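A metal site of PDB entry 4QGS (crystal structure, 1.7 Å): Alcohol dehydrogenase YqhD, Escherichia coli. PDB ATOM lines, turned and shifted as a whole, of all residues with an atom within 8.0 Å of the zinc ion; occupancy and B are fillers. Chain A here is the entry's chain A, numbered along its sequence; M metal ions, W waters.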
ATOM      1  N   ASN A 201      10.637   1.086 -34.560  1.00  0.00           N
ATOM      2  CA  ASN A 201      10.060   1.006 -33.216  1.00  0.00           C
ATOM      3  C   ASN A 201      10.850   1.834 -32.205  1.00  0.00           C
ATOM      4  O   ASN A 201      10.267   2.479 -31.318  1.00  0.00           O
ATOM      5  CB  ASN A 201       9.976  -0.426 -32.708  1.00  0.00           C
ATOM      6  CG  ASN A 201       8.905  -1.240 -33.411  1.00  0.00           C
ATOM      7  OD1 ASN A 201       8.038  -0.697 -34.106  1.00  0.00           O
ATOM      8  ND2 ASN A 201       8.949  -2.559 -33.217  1.00  0.00           N
ATOM      9  N   VAL A 204      10.044   5.534 -32.665  1.00  0.00           N
ATOM     10  CA  VAL A 204       8.726   5.853 -32.134  1.00  0.00           C
ATOM     11  C   VAL A 204       8.716   5.843 -30.601  1.00  0.00           C
ATOM     12  O   VAL A 204       8.182   6.751 -29.961  1.00  0.00           O
ATOM     13  CB  VAL A 204       7.664   4.867 -32.653  1.00  0.00           C
ATOM     14  CG1 VAL A 204       6.341   5.078 -31.923  1.00  0.00           C
ATOM     15  CG2 VAL A 204       7.470   5.079 -34.143  1.00  0.00           C
ATOM     16  N   ASP A 205       9.351   4.833 -30.003  1.00  0.00           N
ATOM     17  CA  ASP A 205       9.348   4.709 -28.551  1.00  0.00           C
ATOM     18  C   ASP A 205      10.088   5.892 -27.921  1.00  0.00           C
ATOM     19  O   ASP A 205       9.588   6.502 -26.956  1.00  0.00           O
ATOM     20  CB  ASP A 205       9.977   3.387 -28.123  1.00  0.00           C
ATOM     21  CG  ASP A 205       9.849   3.118 -26.622  1.00  0.00           C
ATOM     22  OD1 ASP A 205       8.792   3.398 -25.985  1.00  0.00           O
ATOM     23  OD2 ASP A 205      10.844   2.610 -26.063  1.00  0.00           O
ATOM     24  N   ALA A 206      11.241   6.241 -28.476  1.00  0.00           N
ATOM     25  CA  ALA A 206      11.958   7.444 -27.985  1.00  0.00           C
ATOM     26  C   ALA A 206      11.102   8.709 -28.109  1.00  0.00           C
ATOM     27  O   ALA A 206      11.058   9.547 -27.187  1.00  0.00           O
ATOM     28  CB  ALA A 206      13.278   7.614 -28.726  1.00  0.00           C
ATOM     29  N   VAL A 208       7.850   8.974 -28.189  1.00  0.00           N
ATOM     30  CA  VAL A 208       6.737   8.955 -27.260  1.00  0.00           C
ATOM     31  C   VAL A 208       7.212   9.127 -25.824  1.00  0.00           C
ATOM     32  O   VAL A 208       6.578   9.858 -25.063  1.00  0.00           O
ATOM     33  CB  VAL A 208       5.905   7.667 -27.409  1.00  0.00           C
ATOM     34  CG1 VAL A 208       4.816   7.620 -26.348  1.00  0.00           C
ATOM     35  CG2 VAL A 208       5.299   7.633 -28.813  1.00  0.00           C
ATOM     36  N   HIS A 209       8.334   8.500 -25.448  1.00  0.00           N
ATOM     37  CA  HIS A 209       8.868   8.747 -24.088  1.00  0.00           C
ATOM     38  C   HIS A 209       9.084  10.242 -23.867  1.00  0.00           C
ATOM     39  O   HIS A 209       8.827  10.756 -22.774  1.00  0.00           O
ATOM     40  CB  HIS A 209      10.168   7.971 -23.839  1.00  0.00           C
ATOM     41  CG  HIS A 209       9.944   6.551 -23.433  1.00  0.00           C
ATOM     42  ND1 HIS A 209      10.271   6.078 -22.172  1.00  0.00           N
ATOM     43  CD2 HIS A 209       9.392   5.505 -24.098  1.00  0.00           C
ATOM     44  CE1 HIS A 209       9.960   4.795 -22.100  1.00  0.00           C
ATOM     45  NE2 HIS A 209       9.422   4.418 -23.249  1.00  0.00           N
ATOM     46  N   GLU A 212       5.638  12.079 -23.502  1.00  0.00           N
ATOM     47  CA  GLU A 212       4.994  11.694 -22.243  1.00  0.00           C
ATOM     48  C   GLU A 212       5.400  12.660 -21.129  1.00  0.00           C
ATOM     49  O   GLU A 212       4.714  12.754 -20.118  1.00  0.00           O
ATOM     50  CB  GLU A 212       5.373  10.279 -21.820  1.00  0.00           C
ATOM     51  CG  GLU A 212       4.828   9.174 -22.733  1.00  0.00           C
ATOM     52  CD  GLU A 212       3.404   8.726 -22.400  1.00  0.00           C
ATOM     53  OE1 GLU A 212       2.568   9.561 -21.985  1.00  0.00           O
ATOM     54  OE2 GLU A 212       3.139   7.512 -22.540  1.00  0.00           O
ATOM     55  N   GLU A 263      15.168   8.577 -22.943  1.00  0.00           N
ATOM     56  CA  GLU A 263      15.016   7.608 -21.849  1.00  0.00           C
ATOM     57  C   GLU A 263      15.743   7.963 -20.536  1.00  0.00           C
ATOM     58  O   GLU A 263      15.805   7.136 -19.644  1.00  0.00           O
ATOM     59  CB  GLU A 263      15.535   6.257 -22.334  1.00  0.00           C
ATOM     60  CG  GLU A 263      14.472   5.282 -22.787  1.00  0.00           C
ATOM     61  CD  GLU A 263      14.080   5.475 -24.228  1.00  0.00           C
ATOM     62  OE1 GLU A 263      12.869   5.659 -24.502  1.00  0.00           O
ATOM     63  OE2 GLU A 263      14.972   5.445 -25.104  1.00  0.00           O
ATOM     64  N   TRP A 275       2.199   9.457 -19.224  1.00  0.00           N
ATOM     65  CA  TRP A 275       2.399   8.008 -19.295  1.00  0.00           C
ATOM     66  C   TRP A 275       1.123   7.237 -19.545  1.00  0.00           C
ATOM     67  O   TRP A 275       1.146   6.015 -19.570  1.00  0.00           O
ATOM     68  CB  TRP A 275       3.107   7.469 -18.050  1.00  0.00           C
ATOM     69  CG  TRP A 275       4.469   8.083 -17.920  1.00  0.00           C
ATOM     70  CD1 TRP A 275       4.871   8.998 -16.984  1.00  0.00           C
ATOM     71  CD2 TRP A 275       5.577   7.886 -18.804  1.00  0.00           C
ATOM     72  NE1 TRP A 275       6.176   9.367 -17.223  1.00  0.00           N
ATOM     73  CE2 TRP A 275       6.636   8.697 -18.322  1.00  0.00           C
ATOM     74  CE3 TRP A 275       5.796   7.095 -19.936  1.00  0.00           C
ATOM     75  CZ2 TRP A 275       7.883   8.744 -18.945  1.00  0.00           C
ATOM     76  CZ3 TRP A 275       7.025   7.136 -20.553  1.00  0.00           C
ATOM     77  CH2 TRP A 275       8.057   7.954 -20.049  1.00  0.00           C
ATOM     78  N   HIS A 278       1.468   5.096 -22.653  1.00  0.00           N
ATOM     79  CA  HIS A 278       2.139   3.843 -22.295  1.00  0.00           C
ATOM     80  C   HIS A 278       1.227   2.853 -21.571  1.00  0.00           C
ATOM     81  O   HIS A 278       1.227   1.664 -21.910  1.00  0.00           O
ATOM     82  CB  HIS A 278       3.402   4.126 -21.435  1.00  0.00           C
ATOM     83  CG  HIS A 278       4.662   4.225 -22.251  1.00  0.00           C
ATOM     84  ND1 HIS A 278       4.954   5.298 -23.053  1.00  0.00           N
ATOM     85  CD2 HIS A 278       5.689   3.343 -22.424  1.00  0.00           C
ATOM     86  CE1 HIS A 278       6.104   5.095 -23.672  1.00  0.00           C
ATOM     87  NE2 HIS A 278       6.568   3.907 -23.306  1.00  0.00           N
ATOM     88  N   HIS A 282       0.173  -0.684 -23.175  1.00  0.00           N
ATOM     89  CA  HIS A 282       0.634  -1.916 -22.547  1.00  0.00           C
ATOM     90  C   HIS A 282      -0.435  -3.016 -22.602  1.00  0.00           C
ATOM     91  O   HIS A 282      -0.114  -4.180 -22.736  1.00  0.00           O
ATOM     92  CB  HIS A 282       1.045  -1.668 -21.096  1.00  0.00           C
ATOM     93  CG  HIS A 282       2.382  -1.015 -20.935  1.00  0.00           C
ATOM     94  ND1 HIS A 282       2.874  -0.611 -19.708  1.00  0.00           N
ATOM     95  CD2 HIS A 282       3.331  -0.669 -21.847  1.00  0.00           C
ATOM     96  CE1 HIS A 282       4.065  -0.067 -19.866  1.00  0.00           C
ATOM     97  NE2 HIS A 282       4.363  -0.085 -21.146  1.00  0.00           N
ATOM     98  N   HIS A 292       5.620  -3.050 -28.606  1.00  0.00           N
ATOM     99  CA  HIS A 292       5.485  -1.894 -27.718  1.00  0.00           C
ATOM    100  C   HIS A 292       5.237  -0.599 -28.498  1.00  0.00           C
ATOM    101  O   HIS A 292       4.237   0.109 -28.250  1.00  0.00           O
ATOM    102  CB  HIS A 292       6.740  -1.755 -26.853  1.00  0.00           C
ATOM    103  CG  HIS A 292       6.747  -0.556 -25.934  1.00  0.00           C
ATOM    104  ND1 HIS A 292       5.719  -0.295 -25.048  1.00  0.00           N
ATOM    105  CD2 HIS A 292       7.666   0.419 -25.759  1.00  0.00           C
ATOM    106  CE1 HIS A 292       6.010   0.813 -24.373  1.00  0.00           C
ATOM    107  NE2 HIS A 292       7.182   1.267 -24.787  1.00  0.00           N
ATOM    108  N   ALA A 293       6.111  -0.303 -29.445  1.00  0.00           N
ATOM    109  CA  ALA A 293       6.023   0.967 -30.172  1.00  0.00           C
ATOM    110  C   ALA A 293       4.780   1.064 -31.043  1.00  0.00           C
ATOM    111  O   ALA A 293       4.250   2.165 -31.239  1.00  0.00           O
ATOM    112  CB  ALA A 293       7.271   1.172 -31.024  1.00  0.00           C
ATOM    113  N   THR A 295       1.863  -0.101 -30.251  1.00  0.00           N
ATOM    114  CA  THR A 295       0.750   0.272 -29.380  1.00  0.00           C
ATOM    115  C   THR A 295       0.789   1.772 -29.061  1.00  0.00           C
ATOM    116  O   THR A 295      -0.263   2.405 -28.898  1.00  0.00           O
ATOM    117  CB  THR A 295       0.742  -0.522 -28.068  1.00  0.00           C
ATOM    118  OG1 THR A 295       1.812  -0.087 -27.211  1.00  0.00           O
ATOM    119  CG2 THR A 295       0.864  -2.040 -28.358  1.00  0.00           C
ATOM    120  N   LEU A 296       1.995   2.338 -28.972  1.00  0.00           N
ATOM    121  CA  LEU A 296       2.125   3.776 -28.701  1.00  0.00           C
ATOM    122  C   LEU A 296       1.686   4.621 -29.885  1.00  0.00           C
ATOM    123  O   LEU A 296       1.069   5.672 -29.716  1.00  0.00           O
ATOM    124  CB  LEU A 296       3.584   4.125 -28.316  1.00  0.00           C
ATOM    125  CG  LEU A 296       4.207   3.327 -27.166  1.00  0.00           C
ATOM    126  CD1 LEU A 296       5.674   3.766 -26.926  1.00  0.00           C
ATOM    127  CD2 LEU A 296       3.397   3.426 -25.878  1.00  0.00           C
HETATM  128 ZN    ZN M   1       8.312   2.840 -23.991  1.00  0.00          ZN
HETATM  129  O   HOH W   1       8.434   1.887 -22.121  1.00  0.00           O
HETATM  130  O   HOH W   2      10.172   1.751 -24.003  1.00  0.00           O
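ND1 of His 278 is in hydrogen-bond range of OE2 of Glu 212 (2.9 Å).
O of His 292 sits at hydrogen-bond distance from OG1 of Thr 295 (2.6 Å).
Four residues have an atom within 4 Å of the zinc ion: Asp 205, His 209, His 278 and His 292.
The zinc ion is bound by NE2 of His 209 (2.1 Å), NE2 of His 292 (2.1 Å), water W1 (2.1 Å), OD1 of Asp 205 (2.1 Å), water W2 (2.2 Å) and NE2 of His 278 (2.2 Å).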
